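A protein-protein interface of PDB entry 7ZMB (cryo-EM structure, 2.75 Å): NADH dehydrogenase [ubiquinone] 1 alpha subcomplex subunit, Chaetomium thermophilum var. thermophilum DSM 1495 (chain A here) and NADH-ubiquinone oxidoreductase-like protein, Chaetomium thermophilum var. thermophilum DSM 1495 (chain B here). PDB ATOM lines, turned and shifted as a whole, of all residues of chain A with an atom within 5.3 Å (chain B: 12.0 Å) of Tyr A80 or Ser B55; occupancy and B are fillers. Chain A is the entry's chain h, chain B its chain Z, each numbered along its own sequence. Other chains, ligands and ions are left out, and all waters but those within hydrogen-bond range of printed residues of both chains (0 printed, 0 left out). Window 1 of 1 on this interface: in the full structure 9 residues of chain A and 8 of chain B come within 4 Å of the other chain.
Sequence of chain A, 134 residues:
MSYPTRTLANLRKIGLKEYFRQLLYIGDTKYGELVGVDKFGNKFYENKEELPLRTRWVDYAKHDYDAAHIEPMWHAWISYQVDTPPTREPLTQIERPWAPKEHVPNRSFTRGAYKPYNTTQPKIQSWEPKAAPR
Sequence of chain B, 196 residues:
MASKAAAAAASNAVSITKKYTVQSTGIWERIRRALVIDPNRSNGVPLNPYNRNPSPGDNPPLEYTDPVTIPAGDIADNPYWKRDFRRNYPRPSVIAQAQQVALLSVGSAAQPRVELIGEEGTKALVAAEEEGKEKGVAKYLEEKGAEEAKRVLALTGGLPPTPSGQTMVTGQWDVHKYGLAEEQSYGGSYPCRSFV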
ATOM      1  N   LEU A  53     -15.278  17.376  19.086  1.00  0.00           N
ATOM      2  CA  LEU A  53     -15.239  16.388  20.160  1.00  0.00           C
ATOM      3  C   LEU A  53     -14.399  15.175  19.800  1.00  0.00           C
ATOM      4  O   LEU A  53     -14.340  14.219  20.574  1.00  0.00           O
ATOM      5  CB  LEU A  53     -16.639  15.949  20.600  1.00  0.00           C
ATOM      6  CG  LEU A  53     -17.502  17.104  21.099  1.00  0.00           C
ATOM      7  CD1 LEU A  53     -18.820  16.597  21.594  1.00  0.00           C
ATOM      8  CD2 LEU A  53     -16.772  17.888  22.181  1.00  0.00           C
ATOM      9  N   ARG A  54     -13.719  15.199  18.658  1.00  0.00           N
ATOM     10  CA  ARG A  54     -12.806  14.128  18.293  1.00  0.00           C
ATOM     11  C   ARG A  54     -11.362  14.603  18.212  1.00  0.00           C
ATOM     12  O   ARG A  54     -10.479  13.807  17.883  1.00  0.00           O
ATOM     13  CB  ARG A  54     -13.249  13.490  16.974  1.00  0.00           C
ATOM     14  CG  ARG A  54     -14.728  13.170  16.930  1.00  0.00           C
ATOM     15  CD  ARG A  54     -15.045  12.164  15.855  1.00  0.00           C
ATOM     16  NE  ARG A  54     -14.382  10.897  16.120  1.00  0.00           N
ATOM     17  CZ  ARG A  54     -13.884  10.107  15.182  1.00  0.00           C
ATOM     18  NH1 ARG A  54     -13.278   8.979  15.521  1.00  0.00           N
ATOM     19  NH2 ARG A  54     -13.982  10.452  13.909  1.00  0.00           N
ATOM     20  N   THR A  55     -11.094  15.865  18.537  1.00  0.00           N
ATOM     21  CA  THR A  55      -9.741  16.401  18.455  1.00  0.00           C
ATOM     22  C   THR A  55      -8.837  15.887  19.560  1.00  0.00           C
ATOM     23  O   THR A  55      -7.620  15.985  19.433  1.00  0.00           O
ATOM     24  CB  THR A  55      -9.763  17.931  18.492  1.00  0.00           C
ATOM     25  OG1 THR A  55     -10.295  18.373  19.742  1.00  0.00           O
ATOM     26  CG2 THR A  55     -10.613  18.486  17.365  1.00  0.00           C
ATOM     27  N   ARG A  56      -9.399  15.353  20.638  1.00  0.00           N
ATOM     28  CA  ARG A  56      -8.632  14.728  21.702  1.00  0.00           C
ATOM     29  C   ARG A  56      -9.090  13.292  21.859  1.00  0.00           C
ATOM     30  O   ARG A  56     -10.291  13.012  21.849  1.00  0.00           O
ATOM     31  CB  ARG A  56      -8.793  15.474  23.028  1.00  0.00           C
ATOM     32  CG  ARG A  56      -8.253  16.874  23.007  1.00  0.00           C
ATOM     33  CD  ARG A  56      -8.730  17.667  24.183  1.00  0.00           C
ATOM     34  NE  ARG A  56      -8.439  19.084  24.015  1.00  0.00           N
ATOM     35  CZ  ARG A  56      -8.492  19.975  24.993  1.00  0.00           C
ATOM     36  NH1 ARG A  56      -8.823  19.593  26.214  1.00  0.00           N
ATOM     37  NH2 ARG A  56      -8.206  21.238  24.752  1.00  0.00           N
ATOM     38  N   ALA A  76      -9.832  15.441  33.025  1.00  0.00           N
ATOM     39  CA  ALA A  76     -10.376  16.748  32.679  1.00  0.00           C
ATOM     40  C   ALA A  76      -9.964  17.186  31.277  1.00  0.00           C
ATOM     41  O   ALA A  76     -10.736  17.855  30.586  1.00  0.00           O
ATOM     42  CB  ALA A  76      -9.935  17.788  33.709  1.00  0.00           C
ATOM     43  N   TRP A  77      -8.743  16.842  30.853  1.00  0.00           N
ATOM     44  CA  TRP A  77      -8.265  17.233  29.530  1.00  0.00           C
ATOM     45  C   TRP A  77      -8.989  16.474  28.426  1.00  0.00           C
ATOM     46  O   TRP A  77      -9.305  17.047  27.379  1.00  0.00           O
ATOM     47  CB  TRP A  77      -6.754  17.011  29.424  1.00  0.00           C
ATOM     48  CG  TRP A  77      -6.186  17.416  28.095  1.00  0.00           C
ATOM     49  CD1 TRP A  77      -5.802  18.666  27.715  1.00  0.00           C
ATOM     50  CD2 TRP A  77      -5.964  16.572  26.962  1.00  0.00           C
ATOM     51  NE1 TRP A  77      -5.352  18.652  26.425  1.00  0.00           N
ATOM     52  CE2 TRP A  77      -5.442  17.377  25.938  1.00  0.00           C
ATOM     53  CE3 TRP A  77      -6.151  15.210  26.718  1.00  0.00           C
ATOM     54  CZ2 TRP A  77      -5.103  16.868  24.696  1.00  0.00           C
ATOM     55  CZ3 TRP A  77      -5.814  14.711  25.479  1.00  0.00           C
ATOM     56  CH2 TRP A  77      -5.294  15.535  24.488  1.00  0.00           C
ATOM     57  N   ILE A  78      -9.240  15.180  28.628  1.00  0.00           N
ATOM     58  CA  ILE A  78      -9.949  14.394  27.629  1.00  0.00           C
ATOM     59  C   ILE A  78     -11.409  14.810  27.545  1.00  0.00           C
ATOM     60  O   ILE A  78     -12.076  14.542  26.543  1.00  0.00           O
ATOM     61  CB  ILE A  78      -9.800  12.892  27.944  1.00  0.00           C
ATOM     62  CG1 ILE A  78      -9.995  12.042  26.690  1.00  0.00           C
ATOM     63  CG2 ILE A  78     -10.776  12.459  29.013  1.00  0.00           C
ATOM     64  CD1 ILE A  78      -8.996  12.304  25.620  1.00  0.00           C
ATOM     65  N   SER A  79     -11.910  15.489  28.572  1.00  0.00           N
ATOM     66  CA  SER A  79     -13.295  15.906  28.669  1.00  0.00           C
ATOM     67  C   SER A  79     -13.499  17.350  28.257  1.00  0.00           C
ATOM     68  O   SER A  79     -14.598  17.881  28.444  1.00  0.00           O
ATOM     69  CB  SER A  79     -13.795  15.707  30.091  1.00  0.00           C
ATOM     70  OG  SER A  79     -13.792  14.343  30.444  1.00  0.00           O
ATOM     71  N   TYR A  80     -12.465  17.998  27.713  1.00  0.00           N
ATOM     72  CA  TYR A  80     -12.522  19.399  27.301  1.00  0.00           C
ATOM     73  C   TYR A  80     -12.923  20.302  28.455  1.00  0.00           C
ATOM     74  O   TYR A  80     -13.485  21.379  28.254  1.00  0.00           O
ATOM     75  CB  TYR A  80     -13.463  19.605  26.112  1.00  0.00           C
ATOM     76  CG  TYR A  80     -13.093  18.777  24.919  1.00  0.00           C
ATOM     77  CD1 TYR A  80     -12.207  19.252  23.977  1.00  0.00           C
ATOM     78  CD2 TYR A  80     -13.624  17.511  24.741  1.00  0.00           C
ATOM     79  CE1 TYR A  80     -11.862  18.493  22.894  1.00  0.00           C
ATOM     80  CE2 TYR A  80     -13.281  16.746  23.661  1.00  0.00           C
ATOM     81  CZ  TYR A  80     -12.401  17.238  22.742  1.00  0.00           C
ATOM     82  OH  TYR A  80     -12.062  16.472  21.660  1.00  0.00           O
ATOM     83  N   GLN A  81     -12.641  19.859  29.671  1.00  0.00           N
ATOM     84  CA  GLN A  81     -12.876  20.662  30.853  1.00  0.00           C
ATOM     85  C   GLN A  81     -11.726  21.607  31.146  1.00  0.00           C
ATOM     86  O   GLN A  81     -11.904  22.563  31.901  1.00  0.00           O
ATOM     87  CB  GLN A  81     -13.125  19.756  32.058  1.00  0.00           C
ATOM     88  CG  GLN A  81     -13.939  20.414  33.140  1.00  0.00           C
ATOM     89  CD  GLN A  81     -13.901  19.660  34.432  1.00  0.00           C
ATOM     90  OE1 GLN A  81     -12.916  19.008  34.752  1.00  0.00           O
ATOM     91  NE2 GLN A  81     -14.982  19.744  35.193  1.00  0.00           N
ATOM     92  N   VAL A  82     -10.548  21.342  30.588  1.00  0.00           N
ATOM     93  CA  VAL A  82      -9.426  22.267  30.609  1.00  0.00           C
ATOM     94  C   VAL A  82      -8.776  22.206  29.237  1.00  0.00           C
ATOM     95  O   VAL A  82      -8.984  21.266  28.472  1.00  0.00           O
ATOM     96  CB  VAL A  82      -8.399  21.933  31.709  1.00  0.00           C
ATOM     97  CG1 VAL A  82      -8.962  22.253  33.085  1.00  0.00           C
ATOM     98  CG2 VAL A  82      -8.000  20.475  31.624  1.00  0.00           C
ATOM     99  N   ASP A  83      -7.994  23.236  28.916  1.00  0.00           N
ATOM    100  CA  ASP A  83      -7.206  23.208  27.695  1.00  0.00           C
ATOM    101  C   ASP A  83      -5.729  22.959  27.938  1.00  0.00           C
ATOM    102  O   ASP A  83      -5.053  22.462  27.034  1.00  0.00           O
ATOM    103  CB  ASP A  83      -7.366  24.515  26.908  1.00  0.00           C
ATOM    104  CG  ASP A  83      -8.748  24.673  26.312  1.00  0.00           C
ATOM    105  OD1 ASP A  83      -9.211  23.749  25.617  1.00  0.00           O
ATOM    106  OD2 ASP A  83      -9.375  25.725  26.538  1.00  0.00           O
ATOM    107  N   PRO B  46     -20.000  22.253  14.034  1.00  0.00           N
ATOM    108  CA  PRO B  46     -19.456  23.518  14.544  1.00  0.00           C
ATOM    109  C   PRO B  46     -17.974  23.690  14.239  1.00  0.00           C
ATOM    110  O   PRO B  46     -17.281  22.771  13.807  1.00  0.00           O
ATOM    111  CB  PRO B  46     -19.688  23.412  16.057  1.00  0.00           C
ATOM    112  CG  PRO B  46     -20.620  22.267  16.239  1.00  0.00           C
ATOM    113  CD  PRO B  46     -20.334  21.334  15.132  1.00  0.00           C
ATOM    114  N   LEU B  47     -17.494  24.903  14.499  1.00  0.00           N
ATOM    115  CA  LEU B  47     -16.113  25.266  14.205  1.00  0.00           C
ATOM    116  C   LEU B  47     -15.230  25.003  15.415  1.00  0.00           C
ATOM    117  O   LEU B  47     -15.458  25.559  16.491  1.00  0.00           O
ATOM    118  CB  LEU B  47     -16.032  26.728  13.783  1.00  0.00           C
ATOM    119  CG  LEU B  47     -16.904  27.066  12.578  1.00  0.00           C
ATOM    120  CD1 LEU B  47     -17.200  28.534  12.538  1.00  0.00           C
ATOM    121  CD2 LEU B  47     -16.226  26.631  11.320  1.00  0.00           C
ATOM    122  N   ASN B  48     -14.217  24.160  15.233  1.00  0.00           N
ATOM    123  CA  ASN B  48     -13.306  23.850  16.330  1.00  0.00           C
ATOM    124  C   ASN B  48     -12.588  25.071  16.887  1.00  0.00           C
ATOM    125  O   ASN B  48     -12.458  25.156  18.119  1.00  0.00           O
ATOM    126  CB  ASN B  48     -12.306  22.774  15.891  1.00  0.00           C
ATOM    127  CG  ASN B  48     -12.924  21.402  15.854  1.00  0.00           C
ATOM    128  OD1 ASN B  48     -13.711  21.051  16.725  1.00  0.00           O
ATOM    129  ND2 ASN B  48     -12.569  20.610  14.849  1.00  0.00           N
ATOM    130  N   PRO B  49     -12.085  26.015  16.082  1.00  0.00           N
ATOM    131  CA  PRO B  49     -11.457  27.203  16.687  1.00  0.00           C
ATOM    132  C   PRO B  49     -12.416  28.110  17.448  1.00  0.00           C
ATOM    133  O   PRO B  49     -11.989  28.777  18.396  1.00  0.00           O
ATOM    134  CB  PRO B  49     -10.832  27.917  15.478  1.00  0.00           C
ATOM    135  CG  PRO B  49     -11.527  27.373  14.298  1.00  0.00           C
ATOM    136  CD  PRO B  49     -11.851  25.969  14.627  1.00  0.00           C
ATOM    137  N   TYR B  50     -13.694  28.160  17.076  1.00  0.00           N
ATOM    138  CA  TYR B  50     -14.608  29.150  17.643  1.00  0.00           C
ATOM    139  C   TYR B  50     -15.533  28.609  18.721  1.00  0.00           C
ATOM    140  O   TYR B  50     -15.774  29.300  19.712  1.00  0.00           O
ATOM    141  CB  TYR B  50     -15.473  29.772  16.547  1.00  0.00           C
ATOM    142  CG  TYR B  50     -14.696  30.574  15.540  1.00  0.00           C
ATOM    143  CD1 TYR B  50     -13.374  30.929  15.778  1.00  0.00           C
ATOM    144  CD2 TYR B  50     -15.281  30.975  14.351  1.00  0.00           C
ATOM    145  CE1 TYR B  50     -12.666  31.656  14.859  1.00  0.00           C
ATOM    146  CE2 TYR B  50     -14.578  31.702  13.430  1.00  0.00           C
ATOM    147  CZ  TYR B  50     -13.274  32.043  13.688  1.00  0.00           C
ATOM    148  OH  TYR B  50     -12.574  32.774  12.767  1.00  0.00           O
ATOM    149  N   ASN B  51     -16.056  27.400  18.554  1.00  0.00           N
ATOM    150  CA  ASN B  51     -17.062  26.867  19.459  1.00  0.00           C
ATOM    151  C   ASN B  51     -16.411  26.372  20.743  1.00  0.00           C
ATOM    152  O   ASN B  51     -15.585  25.455  20.715  1.00  0.00           O
ATOM    153  CB  ASN B  51     -17.832  25.741  18.779  1.00  0.00           C
ATOM    154  CG  ASN B  51     -19.105  25.400  19.499  1.00  0.00           C
ATOM    155  OD1 ASN B  51     -19.379  24.240  19.773  1.00  0.00           O
ATOM    156  ND2 ASN B  51     -19.893  26.418  19.821  1.00  0.00           N
ATOM    157  N   ARG B  52     -16.790  26.982  21.867  1.00  0.00           N
ATOM    158  CA  ARG B  52     -16.360  26.544  23.190  1.00  0.00           C
ATOM    159  C   ARG B  52     -14.838  26.585  23.317  1.00  0.00           C
ATOM    160  O   ARG B  52     -14.221  25.717  23.936  1.00  0.00           O
ATOM    161  CB  ARG B  52     -16.907  25.146  23.493  1.00  0.00           C
ATOM    162  CG  ARG B  52     -17.252  24.884  24.928  1.00  0.00           C
ATOM    163  CD  ARG B  52     -17.512  23.426  25.120  1.00  0.00           C
ATOM    164  NE  ARG B  52     -17.780  23.055  26.500  1.00  0.00           N
ATOM    165  CZ  ARG B  52     -16.881  22.520  27.315  1.00  0.00           C
ATOM    166  NH1 ARG B  52     -15.650  22.302  26.891  1.00  0.00           N
ATOM    167  NH2 ARG B  52     -17.216  22.203  28.550  1.00  0.00           N
ATOM    168  N   ASN B  53     -14.229  27.609  22.724  1.00  0.00           N
ATOM    169  CA  ASN B  53     -12.778  27.742  22.670  1.00  0.00           C
ATOM    170  C   ASN B  53     -12.436  29.167  23.080  1.00  0.00           C
ATOM    171  O   ASN B  53     -12.704  30.111  22.310  1.00  0.00           O
ATOM    172  CB  ASN B  53     -12.262  27.415  21.267  1.00  0.00           C
ATOM    173  CG  ASN B  53     -10.751  27.301  21.202  1.00  0.00           C
ATOM    174  OD1 ASN B  53     -10.062  27.376  22.212  1.00  0.00           O
ATOM    175  ND2 ASN B  53     -10.234  27.103  20.008  1.00  0.00           N
ATOM    176  N   PRO B  54     -11.857  29.391  24.270  1.00  0.00           N
ATOM    177  CA  PRO B  54     -11.379  28.425  25.265  1.00  0.00           C
ATOM    178  C   PRO B  54     -12.495  27.710  25.999  1.00  0.00           C
ATOM    179  O   PRO B  54     -13.631  28.178  26.021  1.00  0.00           O
ATOM    180  CB  PRO B  54     -10.597  29.298  26.255  1.00  0.00           C
ATOM    181  CG  PRO B  54     -10.499  30.647  25.620  1.00  0.00           C
ATOM    182  CD  PRO B  54     -11.709  30.763  24.764  1.00  0.00           C
ATOM    183  N   SER B  55     -12.162  26.576  26.594  1.00  0.00           N
ATOM    184  CA  SER B  55     -13.097  25.888  27.458  1.00  0.00           C
ATOM    185  C   SER B  55     -13.382  26.741  28.694  1.00  0.00           C
ATOM    186  O   SER B  55     -12.545  27.546  29.107  1.00  0.00           O
ATOM    187  CB  SER B  55     -12.528  24.533  27.865  1.00  0.00           C
ATOM    188  OG  SER B  55     -11.369  24.692  28.665  1.00  0.00           O
ATOM    189  N   PRO B  56     -14.562  26.598  29.300  1.00  0.00           N
ATOM    190  CA  PRO B  56     -14.848  27.366  30.522  1.00  0.00           C
ATOM    191  C   PRO B  56     -13.900  27.048  31.662  1.00  0.00           C
ATOM    192  O   PRO B  56     -13.757  27.871  32.573  1.00  0.00           O
ATOM    193  CB  PRO B  56     -16.291  26.969  30.864  1.00  0.00           C
ATOM    194  CG  PRO B  56     -16.513  25.674  30.152  1.00  0.00           C
ATOM    195  CD  PRO B  56     -15.698  25.750  28.903  1.00  0.00           C
ATOM    196  N   GLY B  57     -13.250  25.884  31.640  1.00  0.00           N
ATOM    197  CA  GLY B  57     -12.281  25.520  32.647  1.00  0.00           C
ATOM    198  C   GLY B  57     -10.929  26.171  32.500  1.00  0.00           C
ATOM    199  O   GLY B  57     -10.065  25.973  33.359  1.00  0.00           O
ATOM    200  N   ASP B  58     -10.719  26.927  31.427  1.00  0.00           N
ATOM    201  CA  ASP B  58      -9.522  27.741  31.279  1.00  0.00           C
ATOM    202  C   ASP B  58      -9.849  29.219  31.116  1.00  0.00           C
ATOM    203  O   ASP B  58      -8.949  30.009  30.823  1.00  0.00           O
ATOM    204  CB  ASP B  58      -8.672  27.246  30.107  1.00  0.00           C
ATOM    205  CG  ASP B  58      -7.619  26.241  30.540  1.00  0.00           C
ATOM    206  OD1 ASP B  58      -7.481  25.997  31.756  1.00  0.00           O
ATOM    207  OD2 ASP B  58      -6.912  25.711  29.668  1.00  0.00           O
ATOM    208  N   ASN B  59     -11.097  29.610  31.302  1.00  0.00           N
ATOM    209  CA  ASN B  59     -11.429  31.021  31.420  1.00  0.00           C
ATOM    210  C   ASN B  59     -10.780  31.557  32.687  1.00  0.00           C
ATOM    211  O   ASN B  59     -10.995  30.988  33.766  1.00  0.00           O
ATOM    212  CB  ASN B  59     -12.939  31.224  31.478  1.00  0.00           C
ATOM    213  CG  ASN B  59     -13.618  30.942  30.166  1.00  0.00           C
ATOM    214  OD1 ASN B  59     -12.982  30.901  29.120  1.00  0.00           O
ATOM    215  ND2 ASN B  59     -14.928  30.744  30.213  1.00  0.00           N
ATOM    216  N   PRO B  60      -9.992  32.669  32.627  1.00  0.00           N
ATOM    217  CA  PRO B  60      -9.407  33.271  33.831  1.00  0.00           C
ATOM    218  C   PRO B  60     -10.424  33.713  34.894  1.00  0.00           C
ATOM    219  O   PRO B  60     -11.372  34.391  34.569  1.00  0.00           O
ATOM    220  CB  PRO B  60      -8.603  34.480  33.330  1.00  0.00           C
ATOM    221  CG  PRO B  60      -9.187  34.786  31.980  1.00  0.00           C
ATOM    222  CD  PRO B  60      -9.552  33.427  31.431  1.00  0.00           C
ATOM    223  N   PRO B  61     -10.226  33.321  36.167  1.00  0.00           N
ATOM    224  CA  PRO B  61     -11.129  33.703  37.251  1.00  0.00           C
ATOM    225  C   PRO B  61     -11.105  35.208  37.526  1.00  0.00           C
ATOM    226  O   PRO B  61     -12.154  35.773  37.775  1.00  0.00           O
ATOM    227  CB  PRO B  61     -10.557  32.991  38.486  1.00  0.00           C
ATOM    228  CG  PRO B  61      -9.619  31.938  37.938  1.00  0.00           C
ATOM    229  CD  PRO B  61      -9.112  32.491  36.625  1.00  0.00           C
ATOM    230  N   GLU B  63     -10.837  37.646  35.632  1.00  0.00           N
ATOM    231  CA  GLU B  63     -11.623  38.462  34.665  1.00  0.00           C
ATOM    232  C   GLU B  63     -13.082  38.648  35.117  1.00  0.00           C
ATOM    233  O   GLU B  63     -13.528  39.797  35.098  1.00  0.00           O
ATOM    234  CB  GLU B  63     -11.525  37.875  33.256  1.00  0.00           C
ATOM    235  CG  GLU B  63     -10.235  38.244  32.548  1.00  0.00           C
ATOM    236  CD  GLU B  63     -10.085  39.722  32.228  1.00  0.00           C
ATOM    237  OE1 GLU B  63     -11.107  40.366  31.918  1.00  0.00           O
ATOM    238  OE2 GLU B  63      -8.947  40.226  32.299  1.00  0.00           O
ATOM    239  N   TYR B  64     -13.808  37.596  35.500  1.00  0.00           N
ATOM    240  CA  TYR B  64     -15.239  37.802  35.872  1.00  0.00           C
ATOM    241  C   TYR B  64     -15.354  38.588  37.182  1.00  0.00           C
ATOM    242  O   TYR B  64     -14.665  38.219  38.110  1.00  0.00           O
ATOM    243  CB  TYR B  64     -15.977  36.476  36.068  1.00  0.00           C
ATOM    244  CG  TYR B  64     -17.367  36.633  36.627  1.00  0.00           C
ATOM    245  CD1 TYR B  64     -18.399  37.091  35.827  1.00  0.00           C
ATOM    246  CD2 TYR B  64     -17.648  36.350  37.953  1.00  0.00           C
ATOM    247  CE1 TYR B  64     -19.677  37.257  36.327  1.00  0.00           C
ATOM    248  CE2 TYR B  64     -18.921  36.513  38.471  1.00  0.00           C
ATOM    249  CZ  TYR B  64     -19.939  36.966  37.651  1.00  0.00           C
ATOM    250  OH  TYR B  64     -21.200  37.130  38.137  1.00  0.00           O
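Of the 12 printed residues of chain A, 5 touch a printed residue of chain B.
Printed residues of chain A that touch a printed residue of chain B: Thr A55, Tyr A80, Gln A81, Val A82 and Asp A83.
Along chain A the printed residues that touch a printed residue of chain B span positions 55 to 83.
Of the 18 printed residues of chain B, 6 touch a printed residue of chain A.
Among the printed residues, 11 pairs touch across the chains.
Among the printed residues, no Asp or Glu carboxylate lies within 4 Å of a Lys or Arg side-chain nitrogen of the other chain.
Among the printed residues, merely in contact across the chains: Gln A81 with Gly B57, Tyr A80 with Ser B55, Asp A83 with Pro B54, Val A82 with Ser B55, Thr A55 with Asn B48, Val A82 with Gly B57, Gln A81 with Ser B55 and Val A82 with Asp B58.
The guanidinium group of Arg B52 is in hydrogen-bond range of the backbone carbonyl oxygen of Tyr A80 (2.7 Å).
The side-chain carboxylate (OD2) of Asp B58 is in hydrogen-bond range of the backbone NH (N) of Asp A83, at 2.8 Å.
The side-chain carboxylate (OD2) of Asp A83 is in hydrogen-bond range of the backbone NH (N) of Ser B55, at 2.9 Å.
Printed residues of chain B within 4 Å of Tyr A80: Arg B52 and Ser B55.
No residue of chain B comes within 4 Å of Leu A53.
Ala A76 touches none of the printed residues of chain B.
No residue of chain B comes within 4 Å of Trp A77.
No residue of chain B comes within 4 Å of Ile A78.
Printed residues of chain B within 4 Å of Gln A81: Ser B55 and Gly B57.
Of chain B, only Pro B54, Ser B55 and Asp B58 come within 4 Å of Asp A83.
Printed residues of chain B within 4 Å of Val A82: Ser B55, Gly B57 and Asp B58.
Printed residues of chain A within 4 Å of Arg B52: Tyr A80.
Of the printed residues of chain A, Asp B58 touches Val A82 (3.99 Å) and Asp A83 (2.8 Å).
Of the printed residues of chain A, Asn B48 touches Thr A55 (3.8 Å).
Of the printed residues of chain A, Gly B57 touches Gln A81 and Val A82.
Leu B47 touches none of the printed residues of chain A.
Glu B63 touches none of the printed residues of chain A.
The nearest printed residue of chain A that does not touch Gly B57 is Asp A83 (5.5 Å).
The backbone carbonyl oxygen (O) of Ser B55 sits close to the side-chain amide oxygen (OD1) of Asn B59, at 3.4 Å.
N of Arg A56 lies within hydrogen-bond range of OH of Tyr A80 (3.1 Å).
The backbone NH (N) of Val A82 sits at hydrogen-bond distance from the backbone carbonyl oxygen (O) of Ala A76, 3.5 Å away.
NH1 of Arg A56 sits at hydrogen-bond distance from O of Val A82, 2.8 Å away.
The backbone carbonyl oxygen (O) of Ala A76 is in hydrogen-bond range of the backbone NH (N) of Gln A81.
OG1 of Thr A55 lies within hydrogen-bond range of OH of Tyr A80 (3.2 Å).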
